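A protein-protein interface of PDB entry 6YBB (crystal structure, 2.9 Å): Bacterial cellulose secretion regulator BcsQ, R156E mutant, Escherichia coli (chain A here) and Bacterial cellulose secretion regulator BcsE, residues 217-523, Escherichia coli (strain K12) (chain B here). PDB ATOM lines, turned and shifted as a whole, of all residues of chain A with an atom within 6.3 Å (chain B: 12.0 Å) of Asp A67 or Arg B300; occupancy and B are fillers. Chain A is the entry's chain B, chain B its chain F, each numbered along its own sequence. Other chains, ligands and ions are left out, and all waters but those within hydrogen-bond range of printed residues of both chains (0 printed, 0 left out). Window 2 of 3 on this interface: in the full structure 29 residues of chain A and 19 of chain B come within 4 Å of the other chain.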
ATOM      1  N   GLY A  57     -18.373 -22.718  31.055  1.00  0.00           N
ATOM      2  CA  GLY A  57     -19.165 -22.707  29.838  1.00  0.00           C
ATOM      3  C   GLY A  57     -18.909 -21.421  29.088  1.00  0.00           C
ATOM      4  O   GLY A  57     -18.300 -20.484  29.614  1.00  0.00           O
ATOM      5  N   TRP A  58     -19.391 -21.381  27.843  1.00  0.00           N
ATOM      6  CA  TRP A  58     -19.052 -20.252  26.982  1.00  0.00           C
ATOM      7  C   TRP A  58     -19.660 -18.957  27.501  1.00  0.00           C
ATOM      8  O   TRP A  58     -18.995 -17.914  27.509  1.00  0.00           O
ATOM      9  CB  TRP A  58     -19.485 -20.518  25.539  1.00  0.00           C
ATOM     10  CG  TRP A  58     -20.961 -20.496  25.278  1.00  0.00           C
ATOM     11  CD1 TRP A  58     -21.796 -21.572  25.220  1.00  0.00           C
ATOM     12  CD2 TRP A  58     -21.773 -19.345  24.998  1.00  0.00           C
ATOM     13  NE1 TRP A  58     -23.078 -21.165  24.938  1.00  0.00           N
ATOM     14  CE2 TRP A  58     -23.091 -19.801  24.798  1.00  0.00           C
ATOM     15  CE3 TRP A  58     -21.516 -17.972  24.908  1.00  0.00           C
ATOM     16  CZ2 TRP A  58     -24.148 -18.938  24.513  1.00  0.00           C
ATOM     17  CZ3 TRP A  58     -22.569 -17.116  24.625  1.00  0.00           C
ATOM     18  CH2 TRP A  58     -23.868 -17.602  24.433  1.00  0.00           C
ATOM     19  N   ALA A  61     -17.848 -17.955  30.582  1.00  0.00           N
ATOM     20  CA  ALA A  61     -16.561 -17.332  30.287  1.00  0.00           C
ATOM     21  C   ALA A  61     -16.731 -15.870  29.884  1.00  0.00           C
ATOM     22  O   ALA A  61     -15.990 -15.001  30.355  1.00  0.00           O
ATOM     23  CB  ALA A  61     -15.836 -18.112  29.191  1.00  0.00           C
ATOM     24  N   MET A  62     -17.701 -15.577  29.012  1.00  0.00           N
ATOM     25  CA  MET A  62     -17.858 -14.209  28.523  1.00  0.00           C
ATOM     26  C   MET A  62     -18.256 -13.253  29.641  1.00  0.00           C
ATOM     27  O   MET A  62     -17.756 -12.125  29.706  1.00  0.00           O
ATOM     28  CB  MET A  62     -18.887 -14.158  27.399  1.00  0.00           C
ATOM     29  CG  MET A  62     -18.429 -14.810  26.127  1.00  0.00           C
ATOM     30  SD  MET A  62     -19.491 -14.399  24.738  1.00  0.00           S
ATOM     31  CE  MET A  62     -18.598 -15.237  23.436  1.00  0.00           C
ATOM     32  N   GLY A  65     -15.409 -12.427  31.729  1.00  0.00           N
ATOM     33  CA  GLY A  65     -14.294 -11.863  30.988  1.00  0.00           C
ATOM     34  C   GLY A  65     -13.212 -12.867  30.652  1.00  0.00           C
ATOM     35  O   GLY A  65     -12.022 -12.538  30.728  1.00  0.00           O
ATOM     36  N   GLN A  66     -13.594 -14.083  30.281  1.00  0.00           N
ATOM     37  CA  GLN A  66     -12.651 -15.142  29.963  1.00  0.00           C
ATOM     38  C   GLN A  66     -12.874 -15.631  28.538  1.00  0.00           C
ATOM     39  O   GLN A  66     -13.882 -15.324  27.896  1.00  0.00           O
ATOM     40  CB  GLN A  66     -12.774 -16.301  30.961  1.00  0.00           C
ATOM     41  CG  GLN A  66     -12.426 -15.916  32.391  1.00  0.00           C
ATOM     42  CD  GLN A  66     -12.397 -17.109  33.323  1.00  0.00           C
ATOM     43  OE1 GLN A  66     -12.781 -18.215  32.942  1.00  0.00           O
ATOM     44  NE2 GLN A  66     -11.936 -16.894  34.551  1.00  0.00           N
ATOM     45  N   ASP A  67     -11.903 -16.396  28.042  1.00  0.00           N
ATOM     46  CA  ASP A  67     -11.956 -16.916  26.683  1.00  0.00           C
ATOM     47  C   ASP A  67     -12.969 -18.052  26.616  1.00  0.00           C
ATOM     48  O   ASP A  67     -12.839 -19.051  27.332  1.00  0.00           O
ATOM     49  CB  ASP A  67     -10.577 -17.395  26.238  1.00  0.00           C
ATOM     50  CG  ASP A  67     -10.413 -17.394  24.726  1.00  0.00           C
ATOM     51  OD1 ASP A  67     -11.437 -17.448  24.009  1.00  0.00           O
ATOM     52  OD2 ASP A  67      -9.258 -17.335  24.253  1.00  0.00           O
ATOM     53  N   TRP A  68     -13.975 -17.899  25.755  1.00  0.00           N
ATOM     54  CA  TRP A  68     -14.983 -18.943  25.610  1.00  0.00           C
ATOM     55  C   TRP A  68     -14.419 -20.178  24.927  1.00  0.00           C
ATOM     56  O   TRP A  68     -14.952 -21.279  25.105  1.00  0.00           O
ATOM     57  CB  TRP A  68     -16.178 -18.411  24.825  1.00  0.00           C
ATOM     58  CG  TRP A  68     -15.826 -17.933  23.451  1.00  0.00           C
ATOM     59  CD1 TRP A  68     -15.460 -16.669  23.090  1.00  0.00           C
ATOM     60  CD2 TRP A  68     -15.804 -18.713  22.252  1.00  0.00           C
ATOM     61  NE1 TRP A  68     -15.215 -16.614  21.739  1.00  0.00           N
ATOM     62  CE2 TRP A  68     -15.419 -17.857  21.202  1.00  0.00           C
ATOM     63  CE3 TRP A  68     -16.074 -20.054  21.963  1.00  0.00           C
ATOM     64  CZ2 TRP A  68     -15.295 -18.297  19.887  1.00  0.00           C
ATOM     65  CZ3 TRP A  68     -15.951 -20.490  20.657  1.00  0.00           C
ATOM     66  CH2 TRP A  68     -15.566 -19.614  19.635  1.00  0.00           C
ATOM     67  N   ARG A  69     -13.354 -20.019  24.139  1.00  0.00           N
ATOM     68  CA  ARG A  69     -12.769 -21.167  23.457  1.00  0.00           C
ATOM     69  C   ARG A  69     -12.169 -22.153  24.445  1.00  0.00           C
ATOM     70  O   ARG A  69     -12.078 -23.350  24.151  1.00  0.00           O
ATOM     71  CB  ARG A  69     -11.720 -20.702  22.448  1.00  0.00           C
ATOM     72  CG  ARG A  69     -12.284 -19.811  21.351  1.00  0.00           C
ATOM     73  CD  ARG A  69     -11.180 -19.245  20.468  1.00  0.00           C
ATOM     74  NE  ARG A  69     -11.665 -18.177  19.595  1.00  0.00           N
ATOM     75  CZ  ARG A  69     -11.809 -16.909  19.972  1.00  0.00           C
ATOM     76  NH1 ARG A  69     -11.511 -16.543  21.214  1.00  0.00           N
ATOM     77  NH2 ARG A  69     -12.256 -16.007  19.111  1.00  0.00           N
ATOM     78  N   ASP A  70     -11.767 -21.677  25.617  1.00  0.00           N
ATOM     79  CA  ASP A  70     -11.223 -22.549  26.645  1.00  0.00           C
ATOM     80  C   ASP A  70     -12.302 -23.260  27.446  1.00  0.00           C
ATOM     81  O   ASP A  70     -11.975 -23.980  28.395  1.00  0.00           O
ATOM     82  CB  ASP A  70     -10.324 -21.747  27.587  1.00  0.00           C
ATOM     83  CG  ASP A  70      -9.026 -21.318  26.929  1.00  0.00           C
ATOM     84  OD1 ASP A  70      -8.466 -22.101  26.132  1.00  0.00           O
ATOM     85  OD2 ASP A  70      -8.559 -20.198  27.215  1.00  0.00           O
ATOM     86  N   ALA A  71     -13.572 -23.070  27.096  1.00  0.00           N
ATOM     87  CA  ALA A  71     -14.680 -23.739  27.760  1.00  0.00           C
ATOM     88  C   ALA A  71     -15.121 -24.995  27.026  1.00  0.00           C
ATOM     89  O   ALA A  71     -16.126 -25.607  27.406  1.00  0.00           O
ATOM     90  CB  ALA A  71     -15.859 -22.775  27.915  1.00  0.00           C
ATOM     91  N   GLY A  72     -14.394 -25.391  25.981  1.00  0.00           N
ATOM     92  CA  GLY A  72     -14.759 -26.567  25.228  1.00  0.00           C
ATOM     93  C   GLY A  72     -14.392 -27.855  25.937  1.00  0.00           C
ATOM     94  O   GLY A  72     -13.579 -27.883  26.860  1.00  0.00           O
ATOM     95  N   ARG A  74     -13.985 -32.283  24.970  1.00  0.00           N
ATOM     96  CA  ARG A  74     -13.897 -33.310  23.940  1.00  0.00           C
ATOM     97  C   ARG A  74     -14.511 -34.601  24.471  1.00  0.00           C
ATOM     98  O   ARG A  74     -14.086 -35.116  25.511  1.00  0.00           O
ATOM     99  CB  ARG A  74     -12.447 -33.536  23.509  1.00  0.00           C
ATOM    100  CG  ARG A  74     -12.293 -34.376  22.243  1.00  0.00           C
ATOM    101  CD  ARG A  74     -10.827 -34.560  21.860  1.00  0.00           C
ATOM    102  NE  ARG A  74     -10.181 -33.289  21.540  1.00  0.00           N
ATOM    103  CZ  ARG A  74     -10.162 -32.747  20.326  1.00  0.00           C
ATOM    104  NH1 ARG A  74     -10.750 -33.368  19.310  1.00  0.00           N
ATOM    105  NH2 ARG A  74      -9.558 -31.586  20.125  1.00  0.00           N
ATOM    106  N   PRO B 296     -15.455 -36.810  29.583  1.00  0.00           N
ATOM    107  CA  PRO B 296     -14.985 -35.735  28.706  1.00  0.00           C
ATOM    108  C   PRO B 296     -13.792 -35.017  29.310  1.00  0.00           C
ATOM    109  O   PRO B 296     -13.655 -34.901  30.530  1.00  0.00           O
ATOM    110  CB  PRO B 296     -16.201 -34.807  28.599  1.00  0.00           C
ATOM    111  CG  PRO B 296     -16.956 -35.044  29.865  1.00  0.00           C
ATOM    112  CD  PRO B 296     -16.768 -36.506  30.177  1.00  0.00           C
ATOM    113  N   GLU B 297     -12.916 -34.539  28.431  1.00  0.00           N
ATOM    114  CA  GLU B 297     -11.721 -33.849  28.869  1.00  0.00           C
ATOM    115  C   GLU B 297     -11.707 -32.426  28.328  1.00  0.00           C
ATOM    116  O   GLU B 297     -12.152 -32.188  27.200  1.00  0.00           O
ATOM    117  CB  GLU B 297     -10.456 -34.593  28.411  1.00  0.00           C
ATOM    118  CG  GLU B 297     -10.303 -35.977  29.025  1.00  0.00           C
ATOM    119  CD  GLU B 297      -9.121 -36.746  28.466  1.00  0.00           C
ATOM    120  OE1 GLU B 297      -8.451 -36.230  27.545  1.00  0.00           O
ATOM    121  OE2 GLU B 297      -8.861 -37.868  28.950  1.00  0.00           O
ATOM    122  N   PRO B 298     -11.217 -31.464  29.106  1.00  0.00           N
ATOM    123  CA  PRO B 298     -11.179 -30.079  28.629  1.00  0.00           C
ATOM    124  C   PRO B 298     -10.235 -29.916  27.450  1.00  0.00           C
ATOM    125  O   PRO B 298      -9.285 -30.678  27.259  1.00  0.00           O
ATOM    126  CB  PRO B 298     -10.684 -29.295  29.849  1.00  0.00           C
ATOM    127  CG  PRO B 298      -9.946 -30.300  30.665  1.00  0.00           C
ATOM    128  CD  PRO B 298     -10.678 -31.592  30.470  1.00  0.00           C
ATOM    129  N   MET B 299     -10.518 -28.891  26.652  1.00  0.00           N
ATOM    130  CA  MET B 299      -9.735 -28.588  25.464  1.00  0.00           C
ATOM    131  C   MET B 299     -10.016 -27.150  25.063  1.00  0.00           C
ATOM    132  O   MET B 299     -11.041 -26.574  25.437  1.00  0.00           O
ATOM    133  CB  MET B 299     -10.076 -29.533  24.310  1.00  0.00           C
ATOM    134  CG  MET B 299     -11.513 -29.400  23.846  1.00  0.00           C
ATOM    135  SD  MET B 299     -11.743 -29.896  22.132  1.00  0.00           S
ATOM    136  CE  MET B 299     -10.648 -28.752  21.299  1.00  0.00           C
ATOM    137  N   ARG B 300      -9.099 -26.576  24.292  1.00  0.00           N
ATOM    138  CA  ARG B 300      -9.299 -25.254  23.719  1.00  0.00           C
ATOM    139  C   ARG B 300      -9.723 -25.397  22.265  1.00  0.00           C
ATOM    140  O   ARG B 300      -9.040 -26.058  21.475  1.00  0.00           O
ATOM    141  CB  ARG B 300      -8.037 -24.397  23.822  1.00  0.00           C
ATOM    142  CG  ARG B 300      -8.149 -23.082  23.070  1.00  0.00           C
ATOM    143  CD  ARG B 300      -6.881 -22.252  23.168  1.00  0.00           C
ATOM    144  NE  ARG B 300      -7.003 -21.017  22.400  1.00  0.00           N
ATOM    145  CZ  ARG B 300      -7.530 -19.894  22.877  1.00  0.00           C
ATOM    146  NH1 ARG B 300      -7.978 -19.849  24.124  1.00  0.00           N
ATOM    147  NH2 ARG B 300      -7.608 -18.815  22.110  1.00  0.00           N
ATOM    148  N   LEU B 301     -10.850 -24.785  21.923  1.00  0.00           N
ATOM    149  CA  LEU B 301     -11.372 -24.842  20.570  1.00  0.00           C
ATOM    150  C   LEU B 301     -10.670 -23.820  19.686  1.00  0.00           C
ATOM    151  O   LEU B 301     -10.170 -22.796  20.159  1.00  0.00           O
ATOM    152  CB  LEU B 301     -12.876 -24.568  20.561  1.00  0.00           C
ATOM    153  CG  LEU B 301     -13.759 -25.243  21.610  1.00  0.00           C
ATOM    154  CD1 LEU B 301     -15.168 -24.699  21.501  1.00  0.00           C
ATOM    155  CD2 LEU B 301     -13.755 -26.758  21.460  1.00  0.00           C
ATOM    156  N   LEU B 302     -10.632 -24.120  18.386  1.00  0.00           N
ATOM    157  CA  LEU B 302     -10.220 -23.155  17.368  1.00  0.00           C
ATOM    158  C   LEU B 302      -8.775 -22.695  17.584  1.00  0.00           C
ATOM    159  O   LEU B 302      -8.481 -21.501  17.663  1.00  0.00           O
ATOM    160  CB  LEU B 302     -11.187 -21.966  17.343  1.00  0.00           C
ATOM    161  CG  LEU B 302     -11.188 -20.989  16.165  1.00  0.00           C
ATOM    162  CD1 LEU B 302     -11.384 -21.719  14.843  1.00  0.00           C
ATOM    163  CD2 LEU B 302     -12.261 -19.920  16.367  1.00  0.00           C
ATOM    164  N   ASP B 303      -7.865 -23.661  17.679  1.00  0.00           N
ATOM    165  CA  ASP B 303      -6.445 -23.352  17.834  1.00  0.00           C
ATOM    166  C   ASP B 303      -5.589 -24.122  16.830  1.00  0.00           C
ATOM    167  O   ASP B 303      -5.547 -23.784  15.647  1.00  0.00           O
ATOM    168  CB  ASP B 303      -5.978 -23.652  19.263  1.00  0.00           C
ATOM    169  CG  ASP B 303      -6.093 -25.122  19.623  1.00  0.00           C
ATOM    170  OD1 ASP B 303      -6.974 -25.809  19.063  1.00  0.00           O
ATOM    171  OD2 ASP B 303      -5.306 -25.589  20.475  1.00  0.00           O
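Of the 8 printed residues of chain B, 7 touch a printed residue of chain A.
Printed residues of chain B that touch a printed residue of chain A: Pro B296, Glu B297, Pro B298, Met B299, Arg B300, Leu B301 and Leu B302.
Hydrophobic or aromatic side chains of chain B that line the printed part of chain A: Pro B296, Met B299, Leu B301 and Leu B302.
Along chain B the printed residues that touch a printed residue of chain A span positions 296 to 302.
Among the printed residues, Asp or Glu carboxylates within 4 Å of a Lys or Arg side-chain nitrogen of the other chain: Asp A67 with Arg B300 (2.8 Å) and Asp A70 with Arg B300 (3.1 Å).
N of Arg A74 sits at hydrogen-bond distance from O of Glu B297 (2.9 Å).
O of Arg A69 sits at hydrogen-bond distance from N of Leu B301, 2.9 Å away.
N of Met B299 lies within hydrogen-bond range of O of Gly A72 (3.2 Å).
The guanidinium group (NH1) of Arg B300 is in salt-bridge range of the side-chain carboxylate (OD1) of Asp A70.
The guanidinium group (NH2) of Arg A74 lies close to the side-chain sulfur (SD) of Met B299.
NH1 of Arg B300 is in salt-bridge range of OD2 of Asp A67 (2.8 Å).
The side-chain carboxylate of Asp A67 lies within salt-bridge range of the guanidinium group of Arg A69 (2.9 Å).
Asp A67 touches just one residue of chain B: Arg B300.
Arg B300 touches just these residues of chain A: Asp A67 (2.8 Å), Arg A69 (3.4 Å) and Asp A70 (3.1 Å).
Gly A57 touches none of the printed residues of chain B.
No residue of chain B comes within 4 Å of Gly A65.
No residue of chain B comes within 4 Å of Gln A66.
Trp A68 touches none of the printed residues of chain B.
Arg A69 touches four residues of chain B.
Of chain B, only Arg B300 comes within 4 Å of Asp A70.
No residue of chain B comes within 4 Å of Ala A71.
Of chain B, only Pro B298, Met B299 and Leu B301 come within 4 Å of Gly A72.
Printed residues of chain A within 4 Å of Pro B296: Arg A74.
Of the printed residues of chain A, Pro B298 touches Gly A72 (3.7 Å).
Of the printed residues of chain A, Leu B302 touches Arg A69 (3.7 Å).
The nearest residue of chain B that does not touch Asp A67 is Leu B301 (6.7 Å).
The nearest printed residue of chain A that does not touch Pro B298 is Arg A74 (5.0 Å).
Arg A69 touches Met B299.
Arg B300 touches Arg A69.
Arg A69 touches Leu B302.
O of Gly A72 touches CA of Pro B298 (3.7 Å).
CA of Gly A72 touches CD2 of Leu B301, 3.9 Å away.
Arg A74 touches Pro B296.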
